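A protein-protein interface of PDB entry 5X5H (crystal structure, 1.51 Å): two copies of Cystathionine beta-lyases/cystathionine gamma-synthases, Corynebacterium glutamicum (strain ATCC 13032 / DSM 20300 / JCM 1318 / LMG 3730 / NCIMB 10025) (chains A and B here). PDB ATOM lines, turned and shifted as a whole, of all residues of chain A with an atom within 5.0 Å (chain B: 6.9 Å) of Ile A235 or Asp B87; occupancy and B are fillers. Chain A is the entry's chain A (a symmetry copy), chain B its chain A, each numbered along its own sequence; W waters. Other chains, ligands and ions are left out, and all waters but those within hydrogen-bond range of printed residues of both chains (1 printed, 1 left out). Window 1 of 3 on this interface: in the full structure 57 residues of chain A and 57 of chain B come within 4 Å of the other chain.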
ATOM      1  N   ASP A  87       7.054  -0.102  -0.142  1.00  0.00           N
ATOM      2  CA  ASP A  87       6.475  -0.118  -1.462  1.00  0.00           C
ATOM      3  C   ASP A  87       5.276   0.791  -1.588  1.00  0.00           C
ATOM      4  O   ASP A  87       5.138   1.567  -2.543  1.00  0.00           O
ATOM      5  CB  ASP A  87       6.107  -1.553  -1.777  1.00  0.00           C
ATOM      6  CG  ASP A  87       5.468  -1.707  -3.119  1.00  0.00           C
ATOM      7  OD1 ASP A  87       6.210  -1.511  -4.138  1.00  0.00           O
ATOM      8  OD2 ASP A  87       4.247  -2.106  -3.271  1.00  0.00           O
ATOM      9  N   ILE A  88       4.391   0.752  -0.619  1.00  0.00           N
ATOM     10  CA  ILE A  88       3.215   1.642  -0.614  1.00  0.00           C
ATOM     11  C   ILE A  88       3.649   3.076  -0.531  1.00  0.00           C
ATOM     12  O   ILE A  88       3.109   3.917  -1.304  1.00  0.00           O
ATOM     13  CB  ILE A  88       2.281   1.311   0.581  1.00  0.00           C
ATOM     14  CG1 ILE A  88       1.614  -0.059   0.425  1.00  0.00           C
ATOM     15  CG2 ILE A  88       1.199   2.385   0.702  1.00  0.00           C
ATOM     16  CD1 ILE A  88       0.805  -0.273  -0.824  1.00  0.00           C
ATOM     17  N   ARG A  91       4.827   4.229  -3.867  1.00  0.00           N
ATOM     18  CA  ARG A  91       3.768   4.348  -4.855  1.00  0.00           C
ATOM     19  C   ARG A  91       2.950   5.546  -4.628  1.00  0.00           C
ATOM     20  O   ARG A  91       2.311   5.968  -5.611  1.00  0.00           O
ATOM     21  CB  ARG A  91       2.959   3.016  -4.886  1.00  0.00           C
ATOM     22  CG  ARG A  91       3.826   1.929  -5.469  1.00  0.00           C
ATOM     23  CD  ARG A  91       3.220   0.594  -5.080  1.00  0.00           C
ATOM     24  NE  ARG A  91       2.220   0.267  -6.052  1.00  0.00           N
ATOM     25  CZ  ARG A  91       1.484  -0.833  -6.044  1.00  0.00           C
ATOM     26  NH1 ARG A  91       1.645  -1.707  -5.088  1.00  0.00           N
ATOM     27  NH2 ARG A  91       0.741  -1.091  -7.094  1.00  0.00           N
ATOM     28  N   PHE A 230      -6.072   4.615   1.560  1.00  0.00           N
ATOM     29  CA  PHE A 230      -6.548   4.238   0.273  1.00  0.00           C
ATOM     30  C   PHE A 230      -5.748   3.069  -0.213  1.00  0.00           C
ATOM     31  O   PHE A 230      -6.284   2.066  -0.708  1.00  0.00           O
ATOM     32  CB  PHE A 230      -6.437   5.400  -0.718  1.00  0.00           C
ATOM     33  CG  PHE A 230      -6.733   5.005  -2.130  1.00  0.00           C
ATOM     34  CD1 PHE A 230      -8.061   4.902  -2.517  1.00  0.00           C
ATOM     35  CD2 PHE A 230      -5.742   4.557  -3.013  1.00  0.00           C
ATOM     36  CE1 PHE A 230      -8.374   4.461  -3.812  1.00  0.00           C
ATOM     37  CE2 PHE A 230      -6.078   4.111  -4.293  1.00  0.00           C
ATOM     38  CZ  PHE A 230      -7.375   4.045  -4.656  1.00  0.00           C
ATOM     39  N   MET A 231      -4.425   3.116  -0.061  1.00  0.00           N
ATOM     40  CA  MET A 231      -3.616   2.046  -0.571  1.00  0.00           C
ATOM     41  C   MET A 231      -3.646   0.768   0.298  1.00  0.00           C
ATOM     42  O   MET A 231      -3.560  -0.362  -0.222  1.00  0.00           O
ATOM     43  CB  MET A 231      -2.130   2.520  -0.727  1.00  0.00           C
ATOM     44  CG  MET A 231      -1.976   3.592  -1.713  1.00  0.00           C
ATOM     45  SD  MET A 231      -2.268   3.186  -3.440  1.00  0.00           S
ATOM     46  CE  MET A 231      -0.601   2.736  -3.921  1.00  0.00           C
ATOM     47  N   GLN A 232      -3.741   0.960   1.606  1.00  0.00           N
ATOM     48  CA  GLN A 232      -3.901  -0.151   2.513  1.00  0.00           C
ATOM     49  C   GLN A 232      -5.061  -1.013   2.031  1.00  0.00           C
ATOM     50  O   GLN A 232      -4.956  -2.238   1.897  1.00  0.00           O
ATOM     51  CB  GLN A 232      -4.158   0.443   3.932  1.00  0.00           C
ATOM     52  CG  GLN A 232      -4.012  -0.567   5.046  1.00  0.00           C
ATOM     53  CD  GLN A 232      -4.282   0.084   6.351  1.00  0.00           C
ATOM     54  OE1 GLN A 232      -5.271   0.767   6.489  1.00  0.00           O
ATOM     55  NE2 GLN A 232      -3.484  -0.164   7.358  1.00  0.00           N
ATOM     56  N   GLY A 233      -6.226  -0.419   1.798  1.00  0.00           N
ATOM     57  CA  GLY A 233      -7.429  -1.085   1.395  1.00  0.00           C
ATOM     58  C   GLY A 233      -7.398  -1.458  -0.072  1.00  0.00           C
ATOM     59  O   GLY A 233      -7.881  -2.508  -0.552  1.00  0.00           O
ATOM     60  N   GLY A 234      -6.789  -0.681  -0.949  1.00  0.00           N
ATOM     61  CA  GLY A 234      -6.915  -0.877  -2.362  1.00  0.00           C
ATOM     62  C   GLY A 234      -5.865  -1.802  -2.940  1.00  0.00           C
ATOM     63  O   GLY A 234      -6.110  -2.504  -3.961  1.00  0.00           O
ATOM     64  N   ILE A 235      -4.653  -1.811  -2.376  1.00  0.00           N
ATOM     65  CA  ILE A 235      -3.628  -2.787  -2.752  1.00  0.00           C
ATOM     66  C   ILE A 235      -3.709  -3.980  -1.745  1.00  0.00           C
ATOM     67  O   ILE A 235      -3.457  -5.121  -2.098  1.00  0.00           O
ATOM     68  CB  ILE A 235      -2.227  -2.194  -2.719  1.00  0.00           C
ATOM     69  CG1 ILE A 235      -2.023  -0.826  -3.392  1.00  0.00           C
ATOM     70  CG2 ILE A 235      -1.116  -3.176  -3.117  1.00  0.00           C
ATOM     71  CD1 ILE A 235      -2.409  -0.763  -4.814  1.00  0.00           C
ATOM     72  N   GLY A 236      -4.053  -3.776  -0.476  1.00  0.00           N
ATOM     73  CA  GLY A 236      -4.272  -4.825   0.459  1.00  0.00           C
ATOM     74  C   GLY A 236      -3.076  -5.506   1.102  1.00  0.00           C
ATOM     75  O   GLY A 236      -3.275  -6.625   1.574  1.00  0.00           O
ATOM     76  N   PRO A 237      -1.914  -4.917   1.334  1.00  0.00           N
ATOM     77  CA  PRO A 237      -0.851  -5.557   2.126  1.00  0.00           C
ATOM     78  C   PRO A 237      -1.099  -5.308   3.586  1.00  0.00           C
ATOM     79  O   PRO A 237      -0.288  -4.558   4.236  1.00  0.00           O
ATOM     80  CB  PRO A 237       0.386  -4.927   1.575  1.00  0.00           C
ATOM     81  CG  PRO A 237       0.030  -3.572   1.260  1.00  0.00           C
ATOM     82  CD  PRO A 237      -1.398  -3.647   0.779  1.00  0.00           C
ATOM     83  N   SER B  81      -3.676 -10.722   0.973  1.00  0.00           N
ATOM     84  CA  SER B  81      -5.088 -10.527   0.598  1.00  0.00           C
ATOM     85  C   SER B  81      -5.174 -10.920  -0.850  1.00  0.00           C
ATOM     86  O   SER B  81      -4.207 -11.006  -1.597  1.00  0.00           O
ATOM     87  CB  SER B  81      -5.577  -9.096   0.882  1.00  0.00           C
ATOM     88  OG  SER B  81      -4.858  -8.208  -0.037  1.00  0.00           O
ATOM     89  N   GLY B  82      -6.410 -11.128  -1.289  1.00  0.00           N
ATOM     90  CA  GLY B  82      -6.727 -11.288  -2.726  1.00  0.00           C
ATOM     91  C   GLY B  82      -6.268 -10.082  -3.536  1.00  0.00           C
ATOM     92  O   GLY B  82      -5.641 -10.239  -4.628  1.00  0.00           O
ATOM     93  N   MET B  83      -6.525  -8.885  -3.035  1.00  0.00           N
ATOM     94  CA  MET B  83      -6.035  -7.709  -3.690  1.00  0.00           C
ATOM     95  C   MET B  83      -4.578  -7.627  -3.816  1.00  0.00           C
ATOM     96  O   MET B  83      -4.015  -7.223  -4.841  1.00  0.00           O
ATOM     97  CB  MET B  83      -6.537  -6.457  -3.005  1.00  0.00           C
ATOM     98  CG  MET B  83      -8.019  -6.158  -3.218  1.00  0.00           C
ATOM     99  SD  MET B  83      -8.605  -6.153  -4.939  1.00  0.00           S
ATOM    100  CE  MET B  83      -7.285  -5.268  -5.736  1.00  0.00           C
ATOM    101  N   ALA B  84      -3.827  -8.020  -2.782  1.00  0.00           N
ATOM    102  CA  ALA B  84      -2.357  -7.926  -2.891  1.00  0.00           C
ATOM    103  C   ALA B  84      -1.827  -8.930  -3.849  1.00  0.00           C
ATOM    104  O   ALA B  84      -0.839  -8.689  -4.590  1.00  0.00           O
ATOM    105  CB  ALA B  84      -1.697  -8.206  -1.535  1.00  0.00           C
ATOM    106  N   ALA B  85      -2.441 -10.125  -3.910  1.00  0.00           N
ATOM    107  CA  ALA B  85      -2.077 -11.161  -4.886  1.00  0.00           C
ATOM    108  C   ALA B  85      -2.306 -10.619  -6.310  1.00  0.00           C
ATOM    109  O   ALA B  85      -1.530 -10.856  -7.230  1.00  0.00           O
ATOM    110  CB  ALA B  85      -2.900 -12.416  -4.619  1.00  0.00           C
ATOM    111  N   THR B  86      -3.442  -9.922  -6.501  1.00  0.00           N
ATOM    112  CA  THR B  86      -3.795  -9.338  -7.833  1.00  0.00           C
ATOM    113  C   THR B  86      -2.725  -8.301  -8.171  1.00  0.00           C
ATOM    114  O   THR B  86      -2.213  -8.287  -9.310  1.00  0.00           O
ATOM    115  CB  THR B  86      -5.183  -8.701  -7.769  1.00  0.00           C
ATOM    116  OG1 THR B  86      -6.181  -9.729  -7.487  1.00  0.00           O
ATOM    117  CG2 THR B  86      -5.586  -8.023  -9.072  1.00  0.00           C
ATOM    118  N   ASP B  87      -2.381  -7.430  -7.259  1.00  0.00           N
ATOM    119  CA  ASP B  87      -1.387  -6.416  -7.514  1.00  0.00           C
ATOM    120  C   ASP B  87      -0.050  -6.994  -7.913  1.00  0.00           C
ATOM    121  O   ASP B  87       0.593  -6.556  -8.877  1.00  0.00           O
ATOM    122  CB  ASP B  87      -1.265  -5.575  -6.260  1.00  0.00           C
ATOM    123  CG  ASP B  87      -0.242  -4.495  -6.384  1.00  0.00           C
ATOM    124  OD1 ASP B  87      -0.504  -3.538  -7.186  1.00  0.00           O
ATOM    125  OD2 ASP B  87       0.829  -4.459  -5.658  1.00  0.00           O
ATOM    126  N   ILE B  88       0.396  -8.011  -7.213  1.00  0.00           N
ATOM    127  CA  ILE B  88       1.661  -8.687  -7.556  1.00  0.00           C
ATOM    128  C   ILE B  88       1.563  -9.313  -8.916  1.00  0.00           C
ATOM    129  O   ILE B  88       2.519  -9.152  -9.727  1.00  0.00           O
ATOM    130  CB  ILE B  88       2.004  -9.776  -6.505  1.00  0.00           C
ATOM    131  CG1 ILE B  88       2.354  -9.169  -5.143  1.00  0.00           C
ATOM    132  CG2 ILE B  88       3.184 -10.615  -6.999  1.00  0.00           C
ATOM    133  CD1 ILE B  88       3.485  -8.179  -5.121  1.00  0.00           C
ATOM    134  N   LEU B  89       0.477 -10.009  -9.263  1.00  0.00           N
ATOM    135  CA  LEU B  89       0.401 -10.638 -10.564  1.00  0.00           C
ATOM    136  C   LEU B  89       0.401  -9.569 -11.638  1.00  0.00           C
ATOM    137  O   LEU B  89       1.101  -9.685 -12.685  1.00  0.00           O
ATOM    138  CB  LEU B  89      -0.839 -11.576 -10.641  1.00  0.00           C
ATOM    139  CG  LEU B  89      -1.019 -12.747 -11.520  1.00  0.00           C
ATOM    140  CD1 LEU B  89       0.224 -13.546 -11.742  1.00  0.00           C
ATOM    141  CD2 LEU B  89      -2.289 -13.411 -11.030  1.00  0.00           C
ATOM    142  N   PHE B  90      -0.266  -8.447 -11.459  1.00  0.00           N
ATOM    143  CA  PHE B  90      -0.283  -7.342 -12.374  1.00  0.00           C
ATOM    144  C   PHE B  90       1.166  -6.859 -12.611  1.00  0.00           C
ATOM    145  O   PHE B  90       1.587  -6.518 -13.743  1.00  0.00           O
ATOM    146  CB  PHE B  90      -1.124  -6.127 -11.973  1.00  0.00           C
ATOM    147  CG  PHE B  90      -2.614  -6.263 -12.086  1.00  0.00           C
ATOM    148  CD1 PHE B  90      -3.271  -7.337 -12.635  1.00  0.00           C
ATOM    149  CD2 PHE B  90      -3.368  -5.286 -11.521  1.00  0.00           C
ATOM    150  CE1 PHE B  90      -4.700  -7.392 -12.675  1.00  0.00           C
ATOM    151  CE2 PHE B  90      -4.760  -5.332 -11.576  1.00  0.00           C
ATOM    152  CZ  PHE B  90      -5.371  -6.363 -12.170  1.00  0.00           C
ATOM    153  N   ARG B  91       1.951  -6.698 -11.536  1.00  0.00           N
ATOM    154  CA  ARG B  91       3.291  -6.142 -11.616  1.00  0.00           C
ATOM    155  C   ARG B  91       4.222  -7.068 -12.273  1.00  0.00           C
ATOM    156  O   ARG B  91       5.249  -6.558 -12.762  1.00  0.00           O
ATOM    157  CB  ARG B  91       3.733  -5.692 -10.190  1.00  0.00           C
ATOM    158  CG  ARG B  91       2.910  -4.498  -9.776  1.00  0.00           C
ATOM    159  CD  ARG B  91       3.018  -4.363  -8.269  1.00  0.00           C
ATOM    160  NE  ARG B  91       4.198  -3.604  -7.980  1.00  0.00           N
ATOM    161  CZ  ARG B  91       4.612  -3.276  -6.767  1.00  0.00           C
ATOM    162  NH1 ARG B  91       3.927  -3.665  -5.726  1.00  0.00           N
ATOM    163  NH2 ARG B  91       5.603  -2.423  -6.658  1.00  0.00           N
ATOM    164  N   ILE B  92       3.997  -8.347 -12.233  1.00  0.00           N
ATOM    165  CA  ILE B  92       4.832  -9.330 -12.934  1.00  0.00           C
ATOM    166  C   ILE B  92       4.522  -9.297 -14.450  1.00  0.00           C
ATOM    167  O   ILE B  92       5.402  -9.261 -15.295  1.00  0.00           O
ATOM    168  CB  ILE B  92       4.608 -10.719 -12.386  1.00  0.00           C
ATOM    169  CG1 ILE B  92       5.216 -10.770 -10.983  1.00  0.00           C
ATOM    170  CG2 ILE B  92       5.221 -11.800 -13.274  1.00  0.00           C
ATOM    171  CD1 ILE B  92       4.772 -11.968 -10.214  1.00  0.00           C
ATOM    172  N   ARG B 112     -10.821  -0.896  -9.542  1.00  0.00           N
ATOM    173  CA  ARG B 112     -10.251   0.270  -8.900  1.00  0.00           C
ATOM    174  C   ARG B 112      -8.751   0.200  -9.004  1.00  0.00           C
ATOM    175  O   ARG B 112      -8.078   1.177  -9.304  1.00  0.00           O
ATOM    176  CB  ARG B 112     -10.715   0.450  -7.478  1.00  0.00           C
ATOM    177  CG  ARG B 112     -10.071   1.614  -6.706  1.00  0.00           C
ATOM    178  CD  ARG B 112     -10.645   1.739  -5.317  1.00  0.00           C
ATOM    179  NE  ARG B 112     -10.854   0.361  -4.791  1.00  0.00           N
ATOM    180  CZ  ARG B 112     -10.616  -0.091  -3.557  1.00  0.00           C
ATOM    181  NH1 ARG B 112     -10.124   0.689  -2.584  1.00  0.00           N
ATOM    182  NH2 ARG B 112     -10.868  -1.362  -3.286  1.00  0.00           N
ATOM    183  N   LEU B 113      -8.190  -0.967  -8.781  1.00  0.00           N
ATOM    184  CA  LEU B 113      -6.734  -1.071  -8.902  1.00  0.00           C
ATOM    185  C   LEU B 113      -6.243  -0.756 -10.279  1.00  0.00           C
ATOM    186  O   LEU B 113      -5.271  -0.018 -10.429  1.00  0.00           O
ATOM    187  CB  LEU B 113      -6.300  -2.516  -8.504  1.00  0.00           C
ATOM    188  CG  LEU B 113      -4.772  -2.816  -8.418  1.00  0.00           C
ATOM    189  CD1 LEU B 113      -4.042  -1.933  -7.473  1.00  0.00           C
ATOM    190  CD2 LEU B 113      -4.561  -4.301  -8.066  1.00  0.00           C
ATOM    191  N   VAL B 117      -4.870   3.083 -10.018  1.00  0.00           N
ATOM    192  CA  VAL B 117      -3.455   2.931  -9.826  1.00  0.00           C
ATOM    193  C   VAL B 117      -2.692   2.604 -11.084  1.00  0.00           C
ATOM    194  O   VAL B 117      -1.763   3.340 -11.471  1.00  0.00           O
ATOM    195  CB  VAL B 117      -3.167   1.847  -8.673  1.00  0.00           C
ATOM    196  CG1 VAL B 117      -1.668   1.618  -8.467  1.00  0.00           C
ATOM    197  CG2 VAL B 117      -3.863   2.294  -7.387  1.00  0.00           C
ATOM    198  N   PHE B 118      -2.988   1.503 -11.780  1.00  0.00           N
ATOM    199  CA  PHE B 118      -2.139   1.091 -12.854  1.00  0.00           C
ATOM    200  C   PHE B 118      -2.157   2.076 -14.057  1.00  0.00           C
ATOM    201  O   PHE B 118      -1.139   2.221 -14.736  1.00  0.00           O
ATOM    202  CB  PHE B 118      -2.331  -0.367 -13.257  1.00  0.00           C
ATOM    203  CG  PHE B 118      -1.639  -1.316 -12.323  1.00  0.00           C
ATOM    204  CD1 PHE B 118      -2.155  -1.521 -11.072  1.00  0.00           C
ATOM    205  CD2 PHE B 118      -0.386  -1.756 -12.619  1.00  0.00           C
ATOM    206  CE1 PHE B 118      -1.493  -2.323 -10.141  1.00  0.00           C
ATOM    207  CE2 PHE B 118       0.291  -2.602 -11.736  1.00  0.00           C
ATOM    208  CZ  PHE B 118      -0.229  -2.804 -10.475  1.00  0.00           C
ATOM    209  N   TRP B 148      -7.989 -10.660 -18.116  1.00  0.00           N
ATOM    210  CA  TRP B 148      -8.414 -10.916 -16.747  1.00  0.00           C
ATOM    211  C   TRP B 148      -9.860 -11.372 -16.732  1.00  0.00           C
ATOM    212  O   TRP B 148     -10.748 -10.582 -17.154  1.00  0.00           O
ATOM    213  CB  TRP B 148      -8.251  -9.659 -15.913  1.00  0.00           C
ATOM    214  CG  TRP B 148      -8.468  -9.952 -14.454  1.00  0.00           C
ATOM    215  CD1 TRP B 148      -9.621  -9.855 -13.737  1.00  0.00           C
ATOM    216  CD2 TRP B 148      -7.445 -10.402 -13.568  1.00  0.00           C
ATOM    217  NE1 TRP B 148      -9.370 -10.189 -12.412  1.00  0.00           N
ATOM    218  CE2 TRP B 148      -8.054 -10.572 -12.322  1.00  0.00           C
ATOM    219  CE3 TRP B 148      -6.065 -10.635 -13.715  1.00  0.00           C
ATOM    220  CZ2 TRP B 148      -7.305 -10.939 -11.190  1.00  0.00           C
ATOM    221  CZ3 TRP B 148      -5.312 -11.046 -12.561  1.00  0.00           C
ATOM    222  CH2 TRP B 148      -5.966 -11.159 -11.331  1.00  0.00           C
ATOM    223  N   LEU B 199      -6.010 -16.970  -9.700  1.00  0.00           N
ATOM    224  CA  LEU B 199      -6.014 -16.158  -8.496  1.00  0.00           C
ATOM    225  C   LEU B 199      -7.166 -16.557  -7.609  1.00  0.00           C
ATOM    226  O   LEU B 199      -8.300 -16.683  -8.083  1.00  0.00           O
ATOM    227  CB  LEU B 199      -6.107 -14.712  -8.900  1.00  0.00           C
ATOM    228  CG  LEU B 199      -6.162 -13.477  -7.962  1.00  0.00           C
ATOM    229  CD1 LEU B 199      -7.414 -13.389  -7.156  1.00  0.00           C
ATOM    230  CD2 LEU B 199      -5.039 -13.294  -7.083  1.00  0.00           C
ATOM    231  N   MET B 231       8.718 -11.564  -5.891  1.00  0.00           N
ATOM    232  CA  MET B 231       7.925 -10.455  -5.442  1.00  0.00           C
ATOM    233  C   MET B 231       7.352 -10.627  -4.018  1.00  0.00           C
ATOM    234  O   MET B 231       7.204  -9.646  -3.264  1.00  0.00           O
ATOM    235  CB  MET B 231       6.742 -10.200  -6.439  1.00  0.00           C
ATOM    236  CG  MET B 231       7.199  -9.804  -7.774  1.00  0.00           C
ATOM    237  SD  MET B 231       7.989  -8.198  -7.943  1.00  0.00           S
ATOM    238  CE  MET B 231       6.549  -7.202  -8.326  1.00  0.00           C
ATOM    239  N   ILE B 235       8.637  -7.379  -2.403  1.00  0.00           N
ATOM    240  CA  ILE B 235       7.622  -6.379  -2.065  1.00  0.00           C
ATOM    241  C   ILE B 235       7.064  -6.721  -0.645  1.00  0.00           C
ATOM    242  O   ILE B 235       6.705  -5.840   0.119  1.00  0.00           O
ATOM    243  CB  ILE B 235       6.476  -6.360  -3.065  1.00  0.00           C
ATOM    244  CG1 ILE B 235       6.842  -6.357  -4.560  1.00  0.00           C
ATOM    245  CG2 ILE B 235       5.389  -5.318  -2.761  1.00  0.00           C
ATOM    246  CD1 ILE B 235       7.714  -5.248  -4.989  1.00  0.00           C
ATOM    247  N   PRO B 237       4.124  -8.539   0.632  1.00  0.00           N
ATOM    248  CA  PRO B 237       2.733  -8.688   1.088  1.00  0.00           C
ATOM    249  C   PRO B 237       2.492 -10.115   1.489  1.00  0.00           C
ATOM    250  O   PRO B 237       1.694 -10.833   0.788  1.00  0.00           O
ATOM    251  CB  PRO B 237       1.952  -8.220  -0.097  1.00  0.00           C
ATOM    252  CG  PRO B 237       2.694  -8.647  -1.249  1.00  0.00           C
ATOM    253  CD  PRO B 237       4.143  -8.522  -0.847  1.00  0.00           C
HETATM  254  O   HOH W   1      -8.547  -1.774  -5.090  1.00  0.00           O
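The side-chain hydroxyl of Ser B81 sits close to the backbone NH of Met B83 (3.5 Å).
The side-chain hydroxyl of Ser B81 sits at hydrogen-bond distance from the backbone NH of Ala B84, at 2.9 Å.
The guanidinium group (NH1) of Arg B91 is in salt-bridge range of the side-chain carboxylate (OD2) of Asp B87 (3.2 Å).
The backbone carbonyl oxygen of Leu B113 sits at hydrogen-bond distance from the backbone NH of Phe B118.
The side-chain carboxylate (OD2) of Asp A87 is in salt-bridge range of the guanidinium group (NH1) of Arg A91 (3.2 Å).
The backbone carbonyl oxygen (O) of Met A231 lies within hydrogen-bond range of the backbone NH (N) of Gly A236, at 3.5 Å.
Of the printed residues of chain B, Asp A87 touches Arg B91 and Ile B235.
Printed residues of chain B within 4 Å of Gly A234: Met B83 and Arg B112.
Ile A235 touches just these residues of chain B: Ser B81, Met B83, Ala B84, Asp B87 and Leu B113.
Printed residues of chain A within 4 Å of Ser B81: Ile A235 and Gly A236.
Of the printed residues of chain A, Met B83 touches Gly A234 and Ile A235.
Asp B87 touches two residues of chain A.
Phe B90 touches none of the printed residues of chain A.
Of the printed residues of chain A, Arg B91 touches Asp A87 (2.7 Å) and Arg A91 (3.1 Å).
Of the printed residues of chain A, Val B117 touches Arg A91.
The nearest residue of chain B that does not touch Ile A235 is Val B117 (4.3 Å).
The nearest residue of chain A that does not touch Asp B87 is Asp A87 (4.8 Å).
The nearest printed residue of chain B that does not touch Arg A91 is Leu B113 (4.9 Å).
Water W1 bridges O of Gly A234 (2.8 Å) and NH2 of Arg B112 (3.0 Å).
Asp A87 touches Ile B235.
CG1 of Val B117 touches NH2 of Arg A91, at 3.9 Å.
NH2 of Arg A91 touches CZ of Phe B118, 3.9 Å away.
CE1 of Phe A230 touches CD of Arg B112, 3.9 Å away.
CE of Met B83 touches O of Gly A234, 3.5 Å away.
Gly A234 touches Arg B112.
Ile A235 touches Ser B81.
O of Ile A235 touches C of Met B83, at 3.2 Å.
Asp B87 touches Ile A235.
O of Gly A236 touches CB of Ala B84, at 3.8 Å.
Asp A87 touches Arg B91, and with the chains exchanged Arg A91 touches Asp B87.
Asp A87 touches Ile B235, and with the chains exchanged Ile A235 touches Asp B87.
Arg A91 touches its own counterpart, Arg B91.
Positions printed for both chains: 87, 88, 91, 231, 235 and 237.
Of the 16 pairs that touch across the chains among the printed residues, 5 have their exchanged pair printed and touching as well.
OG of Ser B81 lies within hydrogen-bond range of O of Gly A236 (2.8 Å).
The backbone carbonyl oxygen (O) of Ile A235 lies within hydrogen-bond range of the backbone NH (N) of Ala B84, 3.0 Å away.
OD1 of Asp B87 is in salt-bridge range of NH2 of Arg A91, 2.7 Å away.
NH2 of Arg B91 is in salt-bridge range of OD1 of Asp A87 (2.7 Å).
The guanidinium group (NH1) of Arg A91 lies close to the guanidinium group (NH1) of Arg B91 (3.1 Å).
Printed residues of chain A that touch a printed residue of chain B: Asp A87, Arg A91, Phe A230, Gly A234, Ile A235 and Gly A236.
Hydrophobic or aromatic side chains of chain A that line the printed part of chain B: Phe A230 and Ile A235.
Of the 21 printed residues of chain B, 10 touch a printed residue of chain A.
Along chain B the printed residues that touch a printed residue of chain A span positions 81 to 235.
Among the printed residues, Asp or Glu carboxylates within 4 Å of a Lys or Arg side-chain nitrogen of the other chain: Asp A87 with Arg B91 and Arg A91 with Asp B87.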
